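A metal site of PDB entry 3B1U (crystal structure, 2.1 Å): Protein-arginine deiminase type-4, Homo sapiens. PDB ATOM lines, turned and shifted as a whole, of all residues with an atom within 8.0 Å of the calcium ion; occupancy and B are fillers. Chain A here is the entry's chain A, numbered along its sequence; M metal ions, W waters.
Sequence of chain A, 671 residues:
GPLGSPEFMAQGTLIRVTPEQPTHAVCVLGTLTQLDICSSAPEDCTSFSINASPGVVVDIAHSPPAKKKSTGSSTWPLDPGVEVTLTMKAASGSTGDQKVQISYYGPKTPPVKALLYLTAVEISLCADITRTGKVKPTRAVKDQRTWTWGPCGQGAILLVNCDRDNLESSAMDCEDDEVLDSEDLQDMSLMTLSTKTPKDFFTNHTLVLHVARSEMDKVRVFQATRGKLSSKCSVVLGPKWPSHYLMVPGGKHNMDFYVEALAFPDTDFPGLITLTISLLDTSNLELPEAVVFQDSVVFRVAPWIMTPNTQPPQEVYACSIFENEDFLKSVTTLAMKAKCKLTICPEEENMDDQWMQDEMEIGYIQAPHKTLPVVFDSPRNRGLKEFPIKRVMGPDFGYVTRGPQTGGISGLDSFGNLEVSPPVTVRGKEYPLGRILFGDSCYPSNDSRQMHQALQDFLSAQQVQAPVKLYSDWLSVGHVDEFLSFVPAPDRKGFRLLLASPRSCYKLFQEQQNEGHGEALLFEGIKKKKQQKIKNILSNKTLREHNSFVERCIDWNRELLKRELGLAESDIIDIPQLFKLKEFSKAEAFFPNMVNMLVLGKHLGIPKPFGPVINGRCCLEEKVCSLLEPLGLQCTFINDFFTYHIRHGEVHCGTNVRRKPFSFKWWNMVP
Water W1 bridges the backbone carbonyl oxygen of Lys 385 (2.6 Å) and the side-chain carboxylate of Asp 377 (2.7 Å). Water W2 lies within hydrogen-bond range of OE1 of Gln 405 (2.6 Å), OG1 of Thr 401 (3.2 Å) and OD2 of Asp 377 (3.5 Å).
The backbone NH (N) of Arg 380 sits close to the side-chain hydroxyl (OG) of Ser 378 (3.2 Å). The backbone carbonyl oxygen (O) of Pro 379 sits close to the side-chain amide nitrogen (ND2) of Asn 381. ND2 of Asn 381 is in hydrogen-bond range of O of Gln 405 (2.7 Å). NE of Arg 380 is in salt-bridge range of OE2 of Glu 359 (2.8 Å). The backbone NH of Arg 382 sits at hydrogen-bond distance from the side-chain carboxylate of Glu 359 (3.3 Å). O of Asp 377 is in hydrogen-bond range of OG1 of Thr 401, at 2.9 Å. OH of Tyr 399 is in hydrogen-bond range of OD2 of Asp 377 (2.6 Å). N of Asp 377 sits at hydrogen-bond distance from O of Val 400 (2.8 Å).
O of Ser 378 binds the calcium ion. OD1 of Asn 381 binds the calcium ion, at 2.3 Å. The calcium ion is bound by water W1 (2.3 Å). The calcium ion is bound by OE1 of Glu 359, at 2.3 Å. The side-chain carboxylate (OD1) of Asp 377 is bound to the calcium ion (2.5 Å). Water W2 binds the calcium ion. The calcium ion has six donor atoms within binding distance.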
ATOM      1  N   ASP A 358       7.759  33.587  -3.967  1.00  0.00           N
ATOM      2  CA  ASP A 358       7.837  32.577  -5.026  1.00  0.00           C
ATOM      3  C   ASP A 358       8.826  31.436  -4.773  1.00  0.00           C
ATOM      4  O   ASP A 358       8.592  30.322  -5.240  1.00  0.00           O
ATOM      5  CB  ASP A 358       8.146  33.272  -6.355  1.00  0.00           C
ATOM      6  CG  ASP A 358       7.002  34.151  -6.833  1.00  0.00           C
ATOM      7  OD1 ASP A 358       5.839  33.932  -6.402  1.00  0.00           O
ATOM      8  OD2 ASP A 358       7.260  35.056  -7.638  1.00  0.00           O
ATOM      9  N   GLU A 359       9.904  31.704  -4.052  1.00  0.00           N
ATOM     10  CA  GLU A 359      10.954  30.705  -3.847  1.00  0.00           C
ATOM     11  C   GLU A 359      10.596  29.676  -2.773  1.00  0.00           C
ATOM     12  O   GLU A 359      11.132  28.557  -2.789  1.00  0.00           O
ATOM     13  CB  GLU A 359      12.283  31.392  -3.481  1.00  0.00           C
ATOM     14  CG  GLU A 359      13.528  30.495  -3.567  1.00  0.00           C
ATOM     15  CD  GLU A 359      13.844  30.024  -4.983  1.00  0.00           C
ATOM     16  OE1 GLU A 359      14.316  28.885  -5.140  1.00  0.00           O
ATOM     17  OE2 GLU A 359      13.637  30.798  -5.946  1.00  0.00           O
ATOM     18  N   MET A 360       9.708  30.020  -1.847  1.00  0.00           N
ATOM     19  CA  MET A 360       9.399  29.130  -0.739  1.00  0.00           C
ATOM     20  C   MET A 360       7.963  29.221  -0.223  1.00  0.00           C
ATOM     21  O   MET A 360       7.241  30.200  -0.483  1.00  0.00           O
ATOM     22  CB  MET A 360      10.346  29.396   0.427  1.00  0.00           C
ATOM     23  CG  MET A 360      10.086  30.707   1.157  1.00  0.00           C
ATOM     24  SD  MET A 360      11.358  31.096   2.371  1.00  0.00           S
ATOM     25  CE  MET A 360      10.649  32.557   3.112  1.00  0.00           C
ATOM     26  N   PHE A 376       9.089  24.571   2.461  1.00  0.00           N
ATOM     27  CA  PHE A 376       9.053  23.893   1.178  1.00  0.00           C
ATOM     28  C   PHE A 376       9.738  24.803   0.171  1.00  0.00           C
ATOM     29  O   PHE A 376       9.231  25.881  -0.138  1.00  0.00           O
ATOM     30  CB  PHE A 376       7.607  23.580   0.778  1.00  0.00           C
ATOM     31  CG  PHE A 376       7.465  22.725  -0.461  1.00  0.00           C
ATOM     32  CD1 PHE A 376       8.541  22.034  -1.014  1.00  0.00           C
ATOM     33  CD2 PHE A 376       6.211  22.598  -1.059  1.00  0.00           C
ATOM     34  CE1 PHE A 376       8.368  21.253  -2.150  1.00  0.00           C
ATOM     35  CE2 PHE A 376       6.042  21.811  -2.187  1.00  0.00           C
ATOM     36  CZ  PHE A 376       7.108  21.133  -2.737  1.00  0.00           C
ATOM     37  N   ASP A 377      10.899  24.373  -0.305  1.00  0.00           N
ATOM     38  CA  ASP A 377      11.726  25.154  -1.207  1.00  0.00           C
ATOM     39  C   ASP A 377      11.338  24.850  -2.655  1.00  0.00           C
ATOM     40  O   ASP A 377      11.420  23.712  -3.096  1.00  0.00           O
ATOM     41  CB  ASP A 377      13.202  24.787  -0.964  1.00  0.00           C
ATOM     42  CG  ASP A 377      14.177  25.687  -1.704  1.00  0.00           C
ATOM     43  OD1 ASP A 377      13.736  26.554  -2.489  1.00  0.00           O
ATOM     44  OD2 ASP A 377      15.397  25.516  -1.489  1.00  0.00           O
ATOM     45  N   SER A 378      10.924  25.883  -3.383  1.00  0.00           N
ATOM     46  CA  SER A 378      10.495  25.727  -4.774  1.00  0.00           C
ATOM     47  C   SER A 378      11.700  25.495  -5.687  1.00  0.00           C
ATOM     48  O   SER A 378      12.763  26.075  -5.468  1.00  0.00           O
ATOM     49  CB  SER A 378       9.743  26.979  -5.261  1.00  0.00           C
ATOM     50  OG  SER A 378       9.539  26.927  -6.662  1.00  0.00           O
ATOM     51  N   PRO A 379      11.526  24.663  -6.733  1.00  0.00           N
ATOM     52  CA  PRO A 379      12.606  24.432  -7.684  1.00  0.00           C
ATOM     53  C   PRO A 379      12.887  25.585  -8.669  1.00  0.00           C
ATOM     54  O   PRO A 379      13.767  25.446  -9.508  1.00  0.00           O
ATOM     55  CB  PRO A 379      12.132  23.203  -8.457  1.00  0.00           C
ATOM     56  CG  PRO A 379      10.656  23.270  -8.387  1.00  0.00           C
ATOM     57  CD  PRO A 379      10.364  23.806  -7.018  1.00  0.00           C
ATOM     58  N   ARG A 380      12.159  26.696  -8.564  1.00  0.00           N
ATOM     59  CA  ARG A 380      12.376  27.821  -9.502  1.00  0.00           C
ATOM     60  C   ARG A 380      13.820  28.338  -9.457  1.00  0.00           C
ATOM     61  O   ARG A 380      14.329  28.813 -10.472  1.00  0.00           O
ATOM     62  CB  ARG A 380      11.358  28.956  -9.275  1.00  0.00           C
ATOM     63  CG  ARG A 380      11.585  29.843  -8.063  1.00  0.00           C
ATOM     64  CD  ARG A 380      11.293  31.310  -8.387  1.00  0.00           C
ATOM     65  NE  ARG A 380      11.639  32.194  -7.272  1.00  0.00           N
ATOM     66  CZ  ARG A 380      11.687  33.521  -7.345  1.00  0.00           C
ATOM     67  NH1 ARG A 380      11.413  34.166  -8.471  1.00  0.00           N
ATOM     68  NH2 ARG A 380      12.011  34.219  -6.263  1.00  0.00           N
ATOM     69  N   ASN A 381      14.452  28.250  -8.285  1.00  0.00           N
ATOM     70  CA  ASN A 381      15.892  28.501  -8.132  1.00  0.00           C
ATOM     71  C   ASN A 381      16.384  29.771  -8.820  1.00  0.00           C
ATOM     72  O   ASN A 381      17.342  29.756  -9.599  1.00  0.00           O
ATOM     73  CB  ASN A 381      16.691  27.279  -8.625  1.00  0.00           C
ATOM     74  CG  ASN A 381      16.458  26.045  -7.775  1.00  0.00           C
ATOM     75  OD1 ASN A 381      15.866  26.121  -6.701  1.00  0.00           O
ATOM     76  ND2 ASN A 381      16.913  24.901  -8.271  1.00  0.00           N
ATOM     77  N   ARG A 382      15.722  30.885  -8.515  1.00  0.00           N
ATOM     78  CA  ARG A 382      16.096  32.185  -9.038  1.00  0.00           C
ATOM     79  C   ARG A 382      17.149  32.802  -8.088  1.00  0.00           C
ATOM     80  O   ARG A 382      17.882  32.068  -7.434  1.00  0.00           O
ATOM     81  CB  ARG A 382      14.853  33.080  -9.196  1.00  0.00           C
ATOM     82  CG  ARG A 382      14.859  33.921 -10.463  1.00  0.00           C
ATOM     83  CD  ARG A 382      14.043  33.284 -11.588  1.00  0.00           C
ATOM     84  NE  ARG A 382      12.636  33.662 -11.521  1.00  0.00           N
ATOM     85  CZ  ARG A 382      12.149  34.863 -11.853  1.00  0.00           C
ATOM     86  NH1 ARG A 382      12.953  35.824 -12.290  1.00  0.00           N
ATOM     87  NH2 ARG A 382      10.856  35.096 -11.753  1.00  0.00           N
ATOM     88  N   LEU A 384      16.886  34.117  -5.205  1.00  0.00           N
ATOM     89  CA  LEU A 384      16.653  33.695  -3.812  1.00  0.00           C
ATOM     90  C   LEU A 384      16.972  32.212  -3.566  1.00  0.00           C
ATOM     91  O   LEU A 384      16.706  31.700  -2.474  1.00  0.00           O
ATOM     92  CB  LEU A 384      15.209  33.986  -3.395  1.00  0.00           C
ATOM     93  CG  LEU A 384      14.835  35.459  -3.164  1.00  0.00           C
ATOM     94  CD1 LEU A 384      13.326  35.610  -3.056  1.00  0.00           C
ATOM     95  CD2 LEU A 384      15.527  36.002  -1.909  1.00  0.00           C
ATOM     96  N   LYS A 385      17.553  31.532  -4.550  1.00  0.00           N
ATOM     97  CA  LYS A 385      17.847  30.084  -4.465  1.00  0.00           C
ATOM     98  C   LYS A 385      18.335  29.624  -3.086  1.00  0.00           C
ATOM     99  O   LYS A 385      17.848  28.623  -2.563  1.00  0.00           O
ATOM    100  CB  LYS A 385      18.894  29.710  -5.523  1.00  0.00           C
ATOM    101  CG  LYS A 385      19.131  28.208  -5.675  1.00  0.00           C
ATOM    102  CD  LYS A 385      20.082  27.907  -6.829  1.00  0.00           C
ATOM    103  CE  LYS A 385      20.325  26.420  -6.987  1.00  0.00           C
ATOM    104  NZ  LYS A 385      21.387  26.125  -7.984  1.00  0.00           N
ATOM    105  N   GLU A 386      19.278  30.355  -2.516  1.00  0.00           N
ATOM    106  CA  GLU A 386      19.960  29.928  -1.279  1.00  0.00           C
ATOM    107  C   GLU A 386      19.242  30.310   0.020  1.00  0.00           C
ATOM    108  O   GLU A 386      19.522  29.710   1.063  1.00  0.00           O
ATOM    109  CB  GLU A 386      21.388  30.477  -1.255  1.00  0.00           C
ATOM    110  CG  GLU A 386      22.294  29.887  -2.340  1.00  0.00           C
ATOM    111  CD  GLU A 386      22.419  28.378  -2.260  1.00  0.00           C
ATOM    112  OE1 GLU A 386      22.287  27.696  -3.303  1.00  0.00           O
ATOM    113  OE2 GLU A 386      22.638  27.860  -1.147  1.00  0.00           O
ATOM    114  N   PHE A 387      18.315  31.266  -0.035  1.00  0.00           N
ATOM    115  CA  PHE A 387      17.668  31.795   1.171  1.00  0.00           C
ATOM    116  C   PHE A 387      17.014  30.731   2.062  1.00  0.00           C
ATOM    117  O   PHE A 387      17.211  30.739   3.277  1.00  0.00           O
ATOM    118  CB  PHE A 387      16.658  32.903   0.813  1.00  0.00           C
ATOM    119  CG  PHE A 387      16.073  33.591   2.017  1.00  0.00           C
ATOM    120  CD1 PHE A 387      16.841  34.481   2.756  1.00  0.00           C
ATOM    121  CD2 PHE A 387      14.759  33.361   2.402  1.00  0.00           C
ATOM    122  CE1 PHE A 387      16.299  35.125   3.863  1.00  0.00           C
ATOM    123  CE2 PHE A 387      14.210  34.004   3.496  1.00  0.00           C
ATOM    124  CZ  PHE A 387      14.991  34.888   4.237  1.00  0.00           C
ATOM    125  N   PRO A 388      16.239  29.793   1.465  1.00  0.00           N
ATOM    126  CA  PRO A 388      15.643  28.731   2.274  1.00  0.00           C
ATOM    127  C   PRO A 388      16.680  27.813   2.922  1.00  0.00           C
ATOM    128  O   PRO A 388      16.462  27.316   4.041  1.00  0.00           O
ATOM    129  CB  PRO A 388      14.780  27.951   1.263  1.00  0.00           C
ATOM    130  CG  PRO A 388      14.593  28.874   0.120  1.00  0.00           C
ATOM    131  CD  PRO A 388      15.847  29.683   0.046  1.00  0.00           C
ATOM    132  N   ILE A 389      17.787  27.582   2.224  1.00  0.00           N
ATOM    133  CA  ILE A 389      18.851  26.690   2.699  1.00  0.00           C
ATOM    134  C   ILE A 389      19.709  27.345   3.781  1.00  0.00           C
ATOM    135  O   ILE A 389      19.965  26.741   4.821  1.00  0.00           O
ATOM    136  CB  ILE A 389      19.761  26.238   1.525  1.00  0.00           C
ATOM    137  CG1 ILE A 389      18.956  25.431   0.510  1.00  0.00           C
ATOM    138  CG2 ILE A 389      20.937  25.417   2.049  1.00  0.00           C
ATOM    139  CD1 ILE A 389      19.757  25.030  -0.726  1.00  0.00           C
ATOM    140  N   TYR A 399      13.353  21.542   6.431  1.00  0.00           N
ATOM    141  CA  TYR A 399      13.552  21.828   5.013  1.00  0.00           C
ATOM    142  C   TYR A 399      13.075  20.656   4.143  1.00  0.00           C
ATOM    143  O   TYR A 399      13.328  19.498   4.457  1.00  0.00           O
ATOM    144  CB  TYR A 399      15.035  22.076   4.728  1.00  0.00           C
ATOM    145  CG  TYR A 399      15.328  22.351   3.268  1.00  0.00           C
ATOM    146  CD1 TYR A 399      15.285  23.648   2.762  1.00  0.00           C
ATOM    147  CD2 TYR A 399      15.624  21.314   2.388  1.00  0.00           C
ATOM    148  CE1 TYR A 399      15.546  23.906   1.427  1.00  0.00           C
ATOM    149  CE2 TYR A 399      15.880  21.556   1.042  1.00  0.00           C
ATOM    150  CZ  TYR A 399      15.834  22.855   0.570  1.00  0.00           C
ATOM    151  OH  TYR A 399      16.088  23.120  -0.754  1.00  0.00           O
ATOM    152  N   VAL A 400      12.385  20.978   3.056  1.00  0.00           N
ATOM    153  CA  VAL A 400      12.039  20.008   2.027  1.00  0.00           C
ATOM    154  C   VAL A 400      12.015  20.680   0.655  1.00  0.00           C
ATOM    155  O   VAL A 400      11.666  21.860   0.544  1.00  0.00           O
ATOM    156  CB  VAL A 400      10.673  19.332   2.296  1.00  0.00           C
ATOM    157  CG1 VAL A 400       9.536  20.339   2.185  1.00  0.00           C
ATOM    158  CG2 VAL A 400      10.450  18.156   1.345  1.00  0.00           C
ATOM    159  N   THR A 401      12.403  19.939  -0.378  1.00  0.00           N
ATOM    160  CA  THR A 401      12.340  20.433  -1.751  1.00  0.00           C
ATOM    161  C   THR A 401      11.948  19.311  -2.707  1.00  0.00           C
ATOM    162  O   THR A 401      12.114  18.126  -2.390  1.00  0.00           O
ATOM    163  CB  THR A 401      13.671  21.034  -2.200  1.00  0.00           C
ATOM    164  OG1 THR A 401      13.492  21.729  -3.435  1.00  0.00           O
ATOM    165  CG2 THR A 401      14.740  19.954  -2.366  1.00  0.00           C
ATOM    166  N   ARG A 402      11.437  19.689  -3.875  1.00  0.00           N
ATOM    167  CA  ARG A 402      10.988  18.720  -4.880  1.00  0.00           C
ATOM    168  C   ARG A 402      11.186  19.257  -6.296  1.00  0.00           C
ATOM    169  O   ARG A 402      11.307  20.470  -6.505  1.00  0.00           O
ATOM    170  CB  ARG A 402       9.516  18.375  -4.677  1.00  0.00           C
ATOM    171  CG  ARG A 402       9.224  17.404  -3.534  1.00  0.00           C
ATOM    172  CD  ARG A 402       9.794  16.019  -3.829  1.00  0.00           C
ATOM    173  NE  ARG A 402       9.411  15.047  -2.807  1.00  0.00           N
ATOM    174  CZ  ARG A 402       9.993  14.918  -1.609  1.00  0.00           C
ATOM    175  NH1 ARG A 402      11.006  15.716  -1.251  1.00  0.00           N
ATOM    176  NH2 ARG A 402       9.560  13.990  -0.770  1.00  0.00           N
ATOM    177  N   GLN A 405      16.168  20.442 -10.266  1.00  0.00           N
ATOM    178  CA  GLN A 405      16.808  21.631  -9.699  1.00  0.00           C
ATOM    179  C   GLN A 405      17.604  22.471 -10.706  1.00  0.00           C
ATOM    180  O   GLN A 405      17.828  23.653 -10.471  1.00  0.00           O
ATOM    181  CB  GLN A 405      17.715  21.210  -8.529  1.00  0.00           C
ATOM    182  CG  GLN A 405      16.967  20.590  -7.353  1.00  0.00           C
ATOM    183  CD  GLN A 405      16.000  21.564  -6.674  1.00  0.00           C
ATOM    184  OE1 GLN A 405      16.279  22.758  -6.585  1.00  0.00           O
ATOM    185  NE2 GLN A 405      14.874  21.046  -6.194  1.00  0.00           N
ATOM    186  N   PHE A 415       5.876  29.659  -5.919  1.00  0.00           N
ATOM    187  CA  PHE A 415       4.895  29.361  -4.870  1.00  0.00           C
ATOM    188  C   PHE A 415       3.913  30.487  -4.539  1.00  0.00           C
ATOM    189  O   PHE A 415       3.152  30.387  -3.573  1.00  0.00           O
ATOM    190  CB  PHE A 415       5.589  28.815  -3.613  1.00  0.00           C
ATOM    191  CG  PHE A 415       6.127  27.400  -3.764  1.00  0.00           C
ATOM    192  CD1 PHE A 415       6.890  26.825  -2.760  1.00  0.00           C
ATOM    193  CD2 PHE A 415       5.882  26.643  -4.921  1.00  0.00           C
ATOM    194  CE1 PHE A 415       7.380  25.535  -2.871  1.00  0.00           C
ATOM    195  CE2 PHE A 415       6.379  25.346  -5.043  1.00  0.00           C
ATOM    196  CZ  PHE A 415       7.126  24.799  -4.018  1.00  0.00           C
HETATM  197 CA    CA M   1      14.795  26.644  -4.711  1.00  0.00          CA
HETATM  198  O   HOH W   1      16.820  26.420  -3.586  1.00  0.00           O
HETATM  199  O   HOH W   2      15.146  24.190  -4.676  1.00  0.00           O
